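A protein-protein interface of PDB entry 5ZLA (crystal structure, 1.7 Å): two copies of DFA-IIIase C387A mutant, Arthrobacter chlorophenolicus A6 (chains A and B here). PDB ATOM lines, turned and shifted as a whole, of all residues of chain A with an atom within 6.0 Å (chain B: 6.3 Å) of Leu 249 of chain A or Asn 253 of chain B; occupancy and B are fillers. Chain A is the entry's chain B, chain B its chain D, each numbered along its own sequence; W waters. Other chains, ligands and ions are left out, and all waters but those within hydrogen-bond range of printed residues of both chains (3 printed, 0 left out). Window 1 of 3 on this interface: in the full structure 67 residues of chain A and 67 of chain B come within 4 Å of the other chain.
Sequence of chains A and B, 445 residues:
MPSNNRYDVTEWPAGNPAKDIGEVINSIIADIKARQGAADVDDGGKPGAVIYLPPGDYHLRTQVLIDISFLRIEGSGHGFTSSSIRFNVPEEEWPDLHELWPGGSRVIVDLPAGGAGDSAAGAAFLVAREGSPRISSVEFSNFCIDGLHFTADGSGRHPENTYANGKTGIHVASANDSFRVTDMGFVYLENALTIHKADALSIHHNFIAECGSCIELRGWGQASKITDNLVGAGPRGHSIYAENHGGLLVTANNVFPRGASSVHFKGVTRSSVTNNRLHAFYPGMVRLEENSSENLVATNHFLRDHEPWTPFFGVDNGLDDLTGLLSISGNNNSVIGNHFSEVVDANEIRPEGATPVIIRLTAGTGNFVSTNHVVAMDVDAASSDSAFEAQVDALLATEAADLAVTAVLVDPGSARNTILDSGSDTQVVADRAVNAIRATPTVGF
Of the 21 printed residues of chain B, 8 touch a printed residue of chain A.
Hydrophobic or aromatic side chains of chain A within 4 Å of the printed part of chain B: Leu 249.
Among the printed residues, 13 pairs touch across the chains.
Among the printed residues, Asp or Glu carboxylates within 4 Å of a Lys or Arg side-chain nitrogen of the other chain: Lys 225 of chain A with Asp 228 of chain B (2.8 Å).
Among the printed residues, pairs that only touch across the chains: Thr 274 of chain A with Asn 275 of chain B (3.2 Å), Gly 247 of chain A with Arg 277 of chain B (3.4 Å), Leu 249 of chain A with Asn 253 of chain B (3.6 Å), Leu 249 of chain A with Ala 252 of chain B (3.6 Å), Lys 225 of chain A with Leu 230 of chain B (3.7 Å), Thr 251 of chain A with Ala 252 of chain B (3.8 Å), Leu 249 of chain A with Asn 275 of chain B (3.9 Å) and Lys 225 of chain A with Asn 229 of chain B (3.96 Å).
6 positions are printed for both chains.
Of chain B, only Ala 252 (3.6 Å), Asn 253 (3.6 Å) and Asn 275 (3.9 Å) come within 4 Å of Leu 249 of chain A.
Asn 253 of chain B touches just one residue of chain A: Leu 249.
Of the printed residues of chain A, Leu 230 of chain B touches Lys 225 (3.7 Å).
Of the printed residues of chain B, Thr 251 of chain A touches Ala 252 (3.8 Å) and Asn 275 (2.5 Å).
Printed residues of chain B within 4 Å of Lys 225 of chain A: Asp 228 (2.7 Å), Asn 229 (3.96 Å) and Leu 230 (3.7 Å).
Printed residues of chain B within 4 Å of Ser 224 of chain A: Asn 254 (3.1 Å).
Printed residues of chain A within 4 Å of Asn 254 of chain B: Ser 224 and Gly 247.
Val 231 of chain B touches none of the printed residues of chain A.
The nearest residue of chain B that does not touch Leu 249 of chain A is Asn 254 of chain B (4.2 Å).
The nearest residue of chain A that does not touch Asn 253 of chain B is Lys 225 of chain A (5.4 Å).
The nearest printed residue of chain A that does not touch Asn 275 of chain B is Ser 272 of chain A (4.3 Å).
Water W2 lies within hydrogen-bond range of the side-chain amide nitrogen of Asn 275 of chain B (2.6 Å), the side-chain hydroxyl of Thr 251 of chain B (3.4 Å) and the side-chain hydroxyl of Thr 251 of chain A (3.5 Å).
Water W1 lies within hydrogen-bond range of the side-chain hydroxyl (OG) of Ser 272 of chain A, the side-chain amide oxygen (OD1) of Asn 275 of chain B and the backbone carbonyl oxygen (O) of Asn 276 of chain B.
Water W3 bridges the side-chain amino group of Lys 225 of chain A (3.1 Å) and the backbone carbonyl oxygen of Asp 228 of chain B (3.3 Å).
N of Ile 226 of chain A lies within hydrogen-bond range of O of Leu 249 of chain A, 2.8 Å away.
The backbone carbonyl oxygen (O) of Ile 226 of chain A lies within hydrogen-bond range of the backbone NH (N) of Thr 251 of chain A (3.0 Å).
The backbone NH of Gly 247 of chain A lies within hydrogen-bond range of the side-chain hydroxyl of Ser 271 of chain A, 3.3 Å away.
The side-chain hydroxyl of Thr 251 of chain A lies within hydrogen-bond range of the backbone carbonyl oxygen of Thr 274 of chain A (2.7 Å).
The side-chain amide oxygen (OD1) of Asn 276 of chain B lies within hydrogen-bond range of the backbone NH (N) of Ala 252 of chain B, at 3.3 Å.
The guanidinium group (NH1) of Arg 277 of chain B sits at hydrogen-bond distance from the side-chain amide oxygen (OD1) of Asn 254 of chain B.
The backbone carbonyl oxygen (O) of Ser 224 of chain A sits at hydrogen-bond distance from the side-chain amide nitrogen (ND2) of Asn 254 of chain B (3.1 Å).
The side-chain amino group (NZ) of Lys 225 of chain A is in salt-bridge range of the side-chain carboxylate (OD1) of Asp 228 of chain B, 2.8 Å away.
The side-chain hydroxyl (OG1) of Thr 227 of chain A is in hydrogen-bond range of the side-chain carboxylate (OD1) of Asp 228 of chain B, 2.6 Å away.
O of Gly 247 of chain A lies within hydrogen-bond range of ND2 of Asn 254 of chain B, at 2.9 Å.
OG1 of Thr 251 of chain A is in hydrogen-bond range of ND2 of Asn 275 of chain B (2.5 Å).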
ATOM      1  N   SER A 224      22.328  -1.607 -35.168  1.00  0.00           N
ATOM      2  CA  SER A 224      23.128  -0.790 -36.074  1.00  0.00           C
ATOM      3  C   SER A 224      23.626   0.470 -35.376  1.00  0.00           C
ATOM      4  O   SER A 224      23.233   0.777 -34.235  1.00  0.00           O
ATOM      5  CB  SER A 224      22.309  -0.457 -37.320  1.00  0.00           C
ATOM      6  OG  SER A 224      21.931  -1.668 -38.009  1.00  0.00           O
ATOM      7  N   LYS A 225      24.525   1.173 -36.058  1.00  0.00           N
ATOM      8  CA  LYS A 225      25.064   2.423 -35.526  1.00  0.00           C
ATOM      9  C   LYS A 225      25.372   3.454 -36.594  1.00  0.00           C
ATOM     10  O   LYS A 225      25.826   3.126 -37.704  1.00  0.00           O
ATOM     11  CB  LYS A 225      26.271   2.188 -34.609  1.00  0.00           C
ATOM     12  CG  LYS A 225      27.487   1.572 -35.241  1.00  0.00           C
ATOM     13  CD  LYS A 225      28.511   1.272 -34.136  1.00  0.00           C
ATOM     14  CE  LYS A 225      29.650   0.420 -34.650  1.00  0.00           C
ATOM     15  NZ  LYS A 225      30.569   1.175 -35.530  1.00  0.00           N
ATOM     16  N   ILE A 226      25.116   4.711 -36.225  1.00  0.00           N
ATOM     17  CA  ILE A 226      25.389   5.886 -37.053  1.00  0.00           C
ATOM     18  C   ILE A 226      26.271   6.790 -36.212  1.00  0.00           C
ATOM     19  O   ILE A 226      25.793   7.415 -35.258  1.00  0.00           O
ATOM     20  CB  ILE A 226      24.068   6.592 -37.434  1.00  0.00           C
ATOM     21  CG1 ILE A 226      23.177   5.634 -38.254  1.00  0.00           C
ATOM     22  CG2 ILE A 226      24.333   7.873 -38.221  1.00  0.00           C
ATOM     23  CD1 ILE A 226      21.798   6.198 -38.513  1.00  0.00           C
ATOM     24  N   THR A 227      27.562   6.829 -36.533  1.00  0.00           N
ATOM     25  CA  THR A 227      28.529   7.494 -35.678  1.00  0.00           C
ATOM     26  C   THR A 227      29.479   8.419 -36.404  1.00  0.00           C
ATOM     27  O   THR A 227      29.954   8.123 -37.486  1.00  0.00           O
ATOM     28  CB  THR A 227      29.368   6.457 -34.885  1.00  0.00           C
ATOM     29  OG1 THR A 227      30.073   5.610 -35.808  1.00  0.00           O
ATOM     30  CG2 THR A 227      28.471   5.616 -33.991  1.00  0.00           C
ATOM     31  N   GLY A 247      17.577  -1.236 -31.059  1.00  0.00           N
ATOM     32  CA  GLY A 247      19.005  -1.237 -30.734  1.00  0.00           C
ATOM     33  C   GLY A 247      19.921  -0.430 -31.653  1.00  0.00           C
ATOM     34  O   GLY A 247      21.087  -0.782 -31.826  1.00  0.00           O
ATOM     35  N   LEU A 248      19.392   0.654 -32.219  1.00  0.00           N
ATOM     36  CA  LEU A 248      20.161   1.604 -33.009  1.00  0.00           C
ATOM     37  C   LEU A 248      20.917   2.545 -32.081  1.00  0.00           C
ATOM     38  O   LEU A 248      20.362   3.008 -31.085  1.00  0.00           O
ATOM     39  CB  LEU A 248      19.217   2.420 -33.898  1.00  0.00           C
ATOM     40  CG  LEU A 248      19.820   3.459 -34.849  1.00  0.00           C
ATOM     41  CD1 LEU A 248      20.792   2.850 -35.854  1.00  0.00           C
ATOM     42  CD2 LEU A 248      18.706   4.203 -35.562  1.00  0.00           C
ATOM     43  N   LEU A 249      22.178   2.814 -32.410  1.00  0.00           N
ATOM     44  CA  LEU A 249      22.986   3.805 -31.682  1.00  0.00           C
ATOM     45  C   LEU A 249      23.347   4.951 -32.617  1.00  0.00           C
ATOM     46  O   LEU A 249      24.011   4.743 -33.632  1.00  0.00           O
ATOM     47  CB  LEU A 249      24.263   3.160 -31.121  1.00  0.00           C
ATOM     48  CG  LEU A 249      25.288   4.082 -30.429  1.00  0.00           C
ATOM     49  CD1 LEU A 249      24.699   4.714 -29.189  1.00  0.00           C
ATOM     50  CD2 LEU A 249      26.505   3.267 -30.050  1.00  0.00           C
ATOM     51  N   VAL A 250      22.904   6.159 -32.275  1.00  0.00           N
ATOM     52  CA  VAL A 250      23.174   7.355 -33.072  1.00  0.00           C
ATOM     53  C   VAL A 250      23.974   8.298 -32.174  1.00  0.00           C
ATOM     54  O   VAL A 250      23.409   8.880 -31.250  1.00  0.00           O
ATOM     55  CB  VAL A 250      21.873   8.047 -33.522  1.00  0.00           C
ATOM     56  CG1 VAL A 250      22.176   9.334 -34.283  1.00  0.00           C
ATOM     57  CG2 VAL A 250      20.999   7.120 -34.358  1.00  0.00           C
ATOM     58  N   THR A 251      25.268   8.437 -32.437  1.00  0.00           N
ATOM     59  CA  THR A 251      26.139   9.159 -31.526  1.00  0.00           C
ATOM     60  C   THR A 251      27.336   9.796 -32.204  1.00  0.00           C
ATOM     61  O   THR A 251      27.791   9.348 -33.252  1.00  0.00           O
ATOM     62  CB  THR A 251      26.591   8.247 -30.350  1.00  0.00           C
ATOM     63  OG1 THR A 251      27.208   9.047 -29.329  1.00  0.00           O
ATOM     64  CG2 THR A 251      27.572   7.172 -30.783  1.00  0.00           C
ATOM     65  N   SER A 271      16.596   2.146 -28.382  1.00  0.00           N
ATOM     66  CA  SER A 271      17.700   2.753 -29.134  1.00  0.00           C
ATOM     67  C   SER A 271      18.226   3.960 -28.378  1.00  0.00           C
ATOM     68  O   SER A 271      17.639   4.390 -27.378  1.00  0.00           O
ATOM     69  CB  SER A 271      17.223   3.150 -30.533  1.00  0.00           C
ATOM     70  OG  SER A 271      16.888   1.992 -31.293  1.00  0.00           O
ATOM     71  N   SER A 272      19.349   4.491 -28.855  1.00  0.00           N
ATOM     72  CA  SER A 272      19.983   5.634 -28.203  1.00  0.00           C
ATOM     73  C   SER A 272      20.394   6.717 -29.208  1.00  0.00           C
ATOM     74  O   SER A 272      21.060   6.430 -30.208  1.00  0.00           O
ATOM     75  CB  SER A 272      21.185   5.156 -27.392  1.00  0.00           C
ATOM     76  OG  SER A 272      21.817   6.245 -26.740  1.00  0.00           O
ATOM     77  N   VAL A 273      19.966   7.947 -28.926  1.00  0.00           N
ATOM     78  CA  VAL A 273      20.349   9.140 -29.669  1.00  0.00           C
ATOM     79  C   VAL A 273      21.048  10.003 -28.643  1.00  0.00           C
ATOM     80  O   VAL A 273      20.398  10.726 -27.876  1.00  0.00           O
ATOM     81  CB  VAL A 273      19.139   9.869 -30.274  1.00  0.00           C
ATOM     82  CG1 VAL A 273      19.593  11.111 -31.029  1.00  0.00           C
ATOM     83  CG2 VAL A 273      18.368   8.958 -31.200  1.00  0.00           C
ATOM     84  N   THR A 274      22.369   9.889 -28.594  1.00  0.00           N
ATOM     85  CA  THR A 274      23.142  10.386 -27.451  1.00  0.00           C
ATOM     86  C   THR A 274      24.416  11.062 -27.910  1.00  0.00           C
ATOM     87  O   THR A 274      25.067  10.616 -28.831  1.00  0.00           O
ATOM     88  CB  THR A 274      23.396   9.226 -26.443  1.00  0.00           C
ATOM     89  OG1 THR A 274      22.135   8.830 -25.877  1.00  0.00           O
ATOM     90  CG2 THR A 274      24.353   9.603 -25.292  1.00  0.00           C
ATOM     91  N   ILE B 203      41.139   0.341 -29.947  1.00  0.00           N
ATOM     92  CA  ILE B 203      40.382  -0.745 -30.589  1.00  0.00           C
ATOM     93  C   ILE B 203      39.132  -0.065 -31.118  1.00  0.00           C
ATOM     94  O   ILE B 203      38.222   0.255 -30.353  1.00  0.00           O
ATOM     95  CB  ILE B 203      40.006  -1.886 -29.619  1.00  0.00           C
ATOM     96  CG1 ILE B 203      41.279  -2.597 -29.139  1.00  0.00           C
ATOM     97  CG2 ILE B 203      39.069  -2.890 -30.310  1.00  0.00           C
ATOM     98  CD1 ILE B 203      41.079  -3.588 -28.017  1.00  0.00           C
ATOM     99  N   ILE B 215      36.791  -9.017 -26.820  1.00  0.00           N
ATOM    100  CA  ILE B 215      37.927  -8.146 -26.445  1.00  0.00           C
ATOM    101  C   ILE B 215      38.308  -8.396 -24.977  1.00  0.00           C
ATOM    102  O   ILE B 215      37.495  -8.170 -24.067  1.00  0.00           O
ATOM    103  CB  ILE B 215      37.607  -6.641 -26.596  1.00  0.00           C
ATOM    104  CG1 ILE B 215      37.246  -6.309 -28.048  1.00  0.00           C
ATOM    105  CG2 ILE B 215      38.776  -5.787 -26.090  1.00  0.00           C
ATOM    106  CD1 ILE B 215      36.549  -4.982 -28.233  1.00  0.00           C
ATOM    107  N   ILE B 226      38.297   1.778 -26.360  1.00  0.00           N
ATOM    108  CA  ILE B 226      37.541   0.768 -27.101  1.00  0.00           C
ATOM    109  C   ILE B 226      36.305   1.520 -27.584  1.00  0.00           C
ATOM    110  O   ILE B 226      35.400   1.825 -26.786  1.00  0.00           O
ATOM    111  CB  ILE B 226      37.142  -0.409 -26.199  1.00  0.00           C
ATOM    112  CG1 ILE B 226      38.384  -1.121 -25.650  1.00  0.00           C
ATOM    113  CG2 ILE B 226      36.238  -1.389 -26.954  1.00  0.00           C
ATOM    114  CD1 ILE B 226      38.072  -2.154 -24.583  1.00  0.00           C
ATOM    115  N   THR B 227      36.293   1.851 -28.875  1.00  0.00           N
ATOM    116  CA  THR B 227      35.286   2.749 -29.436  1.00  0.00           C
ATOM    117  C   THR B 227      34.676   2.262 -30.742  1.00  0.00           C
ATOM    118  O   THR B 227      35.348   1.719 -31.605  1.00  0.00           O
ATOM    119  CB  THR B 227      35.849   4.170 -29.663  1.00  0.00           C
ATOM    120  OG1 THR B 227      36.910   4.124 -30.619  1.00  0.00           O
ATOM    121  CG2 THR B 227      36.385   4.771 -28.364  1.00  0.00           C
ATOM    122  N   ASP B 228      33.376   2.480 -30.883  1.00  0.00           N
ATOM    123  CA  ASP B 228      32.696   2.310 -32.173  1.00  0.00           C
ATOM    124  C   ASP B 228      32.734   0.882 -32.700  1.00  0.00           C
ATOM    125  O   ASP B 228      32.709   0.672 -33.922  1.00  0.00           O
ATOM    126  CB  ASP B 228      33.279   3.298 -33.207  1.00  0.00           C
ATOM    127  CG  ASP B 228      32.213   4.180 -33.833  1.00  0.00           C
ATOM    128  OD1 ASP B 228      31.302   3.673 -34.533  1.00  0.00           O
ATOM    129  OD2 ASP B 228      32.285   5.394 -33.608  1.00  0.00           O
ATOM    130  N   ASN B 229      32.768  -0.100 -31.796  1.00  0.00           N
ATOM    131  CA  ASN B 229      32.769  -1.503 -32.209  1.00  0.00           C
ATOM    132  C   ASN B 229      31.380  -2.122 -32.162  1.00  0.00           C
ATOM    133  O   ASN B 229      30.530  -1.722 -31.370  1.00  0.00           O
ATOM    134  CB  ASN B 229      33.704  -2.345 -31.322  1.00  0.00           C
ATOM    135  CG  ASN B 229      35.122  -1.843 -31.343  1.00  0.00           C
ATOM    136  OD1 ASN B 229      35.859  -2.077 -32.302  1.00  0.00           O
ATOM    137  ND2 ASN B 229      35.514  -1.136 -30.291  1.00  0.00           N
ATOM    138  N   LEU B 230      31.182  -3.104 -33.030  1.00  0.00           N
ATOM    139  CA  LEU B 230      30.038  -4.010 -32.986  1.00  0.00           C
ATOM    140  C   LEU B 230      30.563  -5.324 -32.416  1.00  0.00           C
ATOM    141  O   LEU B 230      31.524  -5.882 -32.944  1.00  0.00           O
ATOM    142  CB  LEU B 230      29.453  -4.205 -34.385  1.00  0.00           C
ATOM    143  CG  LEU B 230      28.478  -3.093 -34.745  1.00  0.00           C
ATOM    144  CD1 LEU B 230      28.466  -2.785 -36.243  1.00  0.00           C
ATOM    145  CD2 LEU B 230      27.080  -3.429 -34.229  1.00  0.00           C
ATOM    146  N   VAL B 231      29.963  -5.773 -31.319  1.00  0.00           N
ATOM    147  CA  VAL B 231      30.502  -6.870 -30.508  1.00  0.00           C
ATOM    148  C   VAL B 231      29.422  -7.849 -30.078  1.00  0.00           C
ATOM    149  O   VAL B 231      28.401  -7.437 -29.533  1.00  0.00           O
ATOM    150  CB  VAL B 231      31.170  -6.330 -29.224  1.00  0.00           C
ATOM    151  CG1 VAL B 231      31.900  -7.444 -28.473  1.00  0.00           C
ATOM    152  CG2 VAL B 231      32.131  -5.196 -29.555  1.00  0.00           C
ATOM    153  N   ILE B 240      33.461  -7.338 -23.684  1.00  0.00           N
ATOM    154  CA  ILE B 240      34.579  -6.442 -23.403  1.00  0.00           C
ATOM    155  C   ILE B 240      35.017  -6.719 -21.966  1.00  0.00           C
ATOM    156  O   ILE B 240      34.206  -6.631 -21.037  1.00  0.00           O
ATOM    157  CB  ILE B 240      34.177  -4.959 -23.549  1.00  0.00           C
ATOM    158  CG1 ILE B 240      33.821  -4.658 -25.002  1.00  0.00           C
ATOM    159  CG2 ILE B 240      35.326  -4.057 -23.077  1.00  0.00           C
ATOM    160  CD1 ILE B 240      33.163  -3.321 -25.246  1.00  0.00           C
ATOM    161  N   LEU B 249      38.706   4.223 -21.755  1.00  0.00           N
ATOM    162  CA  LEU B 249      37.465   4.807 -22.272  1.00  0.00           C
ATOM    163  C   LEU B 249      36.768   3.779 -23.149  1.00  0.00           C
ATOM    164  O   LEU B 249      37.322   3.385 -24.165  1.00  0.00           O
ATOM    165  CB  LEU B 249      37.775   6.058 -23.089  1.00  0.00           C
ATOM    166  CG  LEU B 249      36.575   6.778 -23.726  1.00  0.00           C
ATOM    167  CD1 LEU B 249      35.554   7.260 -22.699  1.00  0.00           C
ATOM    168  CD2 LEU B 249      37.114   7.939 -24.548  1.00  0.00           C
ATOM    169  N   VAL B 250      35.564   3.368 -22.759  1.00  0.00           N
ATOM    170  CA  VAL B 250      34.758   2.396 -23.502  1.00  0.00           C
ATOM    171  C   VAL B 250      33.480   3.125 -23.916  1.00  0.00           C
ATOM    172  O   VAL B 250      32.626   3.396 -23.073  1.00  0.00           O
ATOM    173  CB  VAL B 250      34.396   1.172 -22.622  1.00  0.00           C
ATOM    174  CG1 VAL B 250      33.569   0.162 -23.413  1.00  0.00           C
ATOM    175  CG2 VAL B 250      35.658   0.516 -22.064  1.00  0.00           C
ATOM    176  N   THR B 251      33.376   3.490 -25.198  1.00  0.00           N
ATOM    177  CA  THR B 251      32.265   4.316 -25.671  1.00  0.00           C
ATOM    178  C   THR B 251      31.851   4.038 -27.116  1.00  0.00           C
ATOM    179  O   THR B 251      32.638   3.574 -27.935  1.00  0.00           O
ATOM    180  CB  THR B 251      32.574   5.825 -25.460  1.00  0.00           C
ATOM    181  OG1 THR B 251      31.377   6.603 -25.635  1.00  0.00           O
ATOM    182  CG2 THR B 251      33.635   6.332 -26.412  1.00  0.00           C
ATOM    183  N   ALA B 252      30.582   4.321 -27.395  1.00  0.00           N
ATOM    184  CA  ALA B 252      30.010   4.254 -28.738  1.00  0.00           C
ATOM    185  C   ALA B 252      30.053   2.833 -29.318  1.00  0.00           C
ATOM    186  O   ALA B 252      30.084   2.641 -30.531  1.00  0.00           O
ATOM    187  CB  ALA B 252      30.670   5.271 -29.658  1.00  0.00           C
ATOM    188  N   ASN B 253      30.054   1.828 -28.441  1.00  0.00           N
ATOM    189  CA  ASN B 253      30.012   0.443 -28.892  1.00  0.00           C
ATOM    190  C   ASN B 253      28.561  -0.011 -28.913  1.00  0.00           C
ATOM    191  O   ASN B 253      27.743   0.446 -28.105  1.00  0.00           O
ATOM    192  CB  ASN B 253      30.838  -0.454 -27.987  1.00  0.00           C
ATOM    193  CG  ASN B 253      32.288  -0.038 -27.939  1.00  0.00           C
ATOM    194  OD1 ASN B 253      33.029  -0.260 -28.886  1.00  0.00           O
ATOM    195  ND2 ASN B 253      32.699   0.583 -26.845  1.00  0.00           N
ATOM    196  N   ASN B 254      28.260  -0.883 -29.866  1.00  0.00           N
ATOM    197  CA  ASN B 254      26.983  -1.580 -29.915  1.00  0.00           C
ATOM    198  C   ASN B 254      27.276  -3.045 -29.618  1.00  0.00           C
ATOM    199  O   ASN B 254      27.811  -3.783 -30.480  1.00  0.00           O
ATOM    200  CB  ASN B 254      26.327  -1.394 -31.272  1.00  0.00           C
ATOM    201  CG  ASN B 254      24.883  -1.818 -31.271  1.00  0.00           C
ATOM    202  OD1 ASN B 254      24.529  -2.867 -30.709  1.00  0.00           O
ATOM    203  ND2 ASN B 254      24.020  -0.984 -31.844  1.00  0.00           N
ATOM    204  N   VAL B 255      27.009  -3.417 -28.368  1.00  0.00           N
ATOM    205  CA  VAL B 255      27.269  -4.760 -27.852  1.00  0.00           C
ATOM    206  C   VAL B 255      25.939  -5.496 -27.839  1.00  0.00           C
ATOM    207  O   VAL B 255      25.019  -5.114 -27.117  1.00  0.00           O
ATOM    208  CB  VAL B 255      27.865  -4.739 -26.430  1.00  0.00           C
ATOM    209  CG1 VAL B 255      28.216  -6.157 -25.975  1.00  0.00           C
ATOM    210  CG2 VAL B 255      29.107  -3.867 -26.391  1.00  0.00           C
ATOM    211  N   THR B 274      30.688   4.651 -21.123  1.00  0.00           N
ATOM    212  CA  THR B 274      29.734   5.709 -21.346  1.00  0.00           C
ATOM    213  C   THR B 274      29.227   5.677 -22.767  1.00  0.00           C
ATOM    214  O   THR B 274      29.982   5.425 -23.705  1.00  0.00           O
ATOM    215  CB  THR B 274      30.400   7.057 -20.983  1.00  0.00           C
ATOM    216  OG1 THR B 274      30.600   7.065 -19.569  1.00  0.00           O
ATOM    217  CG2 THR B 274      29.564   8.272 -21.385  1.00  0.00           C
ATOM    218  N   ASN B 275      27.938   5.925 -22.921  1.00  0.00           N
ATOM    219  CA  ASN B 275      27.335   6.023 -24.232  1.00  0.00           C
ATOM    220  C   ASN B 275      27.531   4.766 -25.091  1.00  0.00           C
ATOM    221  O   ASN B 275      27.925   4.851 -26.251  1.00  0.00           O
ATOM    222  CB  ASN B 275      27.868   7.263 -24.952  1.00  0.00           C
ATOM    223  CG  ASN B 275      27.252   7.446 -26.306  1.00  0.00           C
ATOM    224  OD1 ASN B 275      26.067   7.128 -26.513  1.00  0.00           O
ATOM    225  ND2 ASN B 275      28.049   7.878 -27.253  1.00  0.00           N
ATOM    226  N   ASN B 276      27.241   3.605 -24.513  1.00  0.00           N
ATOM    227  CA  ASN B 276      27.214   2.361 -25.275  1.00  0.00           C
ATOM    228  C   ASN B 276      25.794   1.876 -25.350  1.00  0.00           C
ATOM    229  O   ASN B 276      24.979   2.212 -24.499  1.00  0.00           O
ATOM    230  CB  ASN B 276      28.066   1.280 -24.610  1.00  0.00           C
ATOM    231  CG  ASN B 276      29.512   1.690 -24.488  1.00  0.00           C
ATOM    232  OD1 ASN B 276      30.266   1.619 -25.444  1.00  0.00           O
ATOM    233  ND2 ASN B 276      29.892   2.149 -23.320  1.00  0.00           N
ATOM    234  N   ARG B 277      25.501   1.107 -26.390  1.00  0.00           N
ATOM    235  CA  ARG B 277      24.251   0.360 -26.467  1.00  0.00           C
ATOM    236  C   ARG B 277      24.618  -1.073 -26.120  1.00  0.00           C
ATOM    237  O   ARG B 277      25.487  -1.672 -26.770  1.00  0.00           O
ATOM    238  CB  ARG B 277      23.629   0.471 -27.856  1.00  0.00           C
ATOM    239  CG  ARG B 277      22.288  -0.244 -27.987  1.00  0.00           C
ATOM    240  CD  ARG B 277      22.478  -1.653 -28.507  1.00  0.00           C
ATOM    241  NE  ARG B 277      21.239  -2.421 -28.533  1.00  0.00           N
ATOM    242  CZ  ARG B 277      21.036  -3.536 -29.238  1.00  0.00           C
ATOM    243  NH1 ARG B 277      21.985  -4.068 -30.014  1.00  0.00           N
ATOM    244  NH2 ARG B 277      19.842  -4.133 -29.159  1.00  0.00           N
ATOM    245  N   LEU B 278      23.950  -1.604 -25.098  1.00  0.00           N
ATOM    246  CA  LEU B 278      24.268  -2.915 -24.521  1.00  0.00           C
ATOM    247  C   LEU B 278      23.010  -3.751 -24.487  1.00  0.00           C
ATOM    248  O   LEU B 278      22.030  -3.334 -23.879  1.00  0.00           O
ATOM    249  CB  LEU B 278      24.781  -2.743 -23.099  1.00  0.00           C
ATOM    250  CG  LEU B 278      25.933  -1.755 -22.900  1.00  0.00           C
ATOM    251  CD1 LEU B 278      26.249  -1.605 -21.419  1.00  0.00           C
ATOM    252  CD2 LEU B 278      27.182  -2.137 -23.672  1.00  0.00           C
HETATM  253  O   HOH W   1      24.019   5.405 -25.321  1.00  0.00           O
HETATM  254  O   HOH W   2      30.255   9.081 -27.700  1.00  0.00           O
HETATM  255  O   HOH W   3      32.180  -1.259 -36.529  1.00  0.00           O
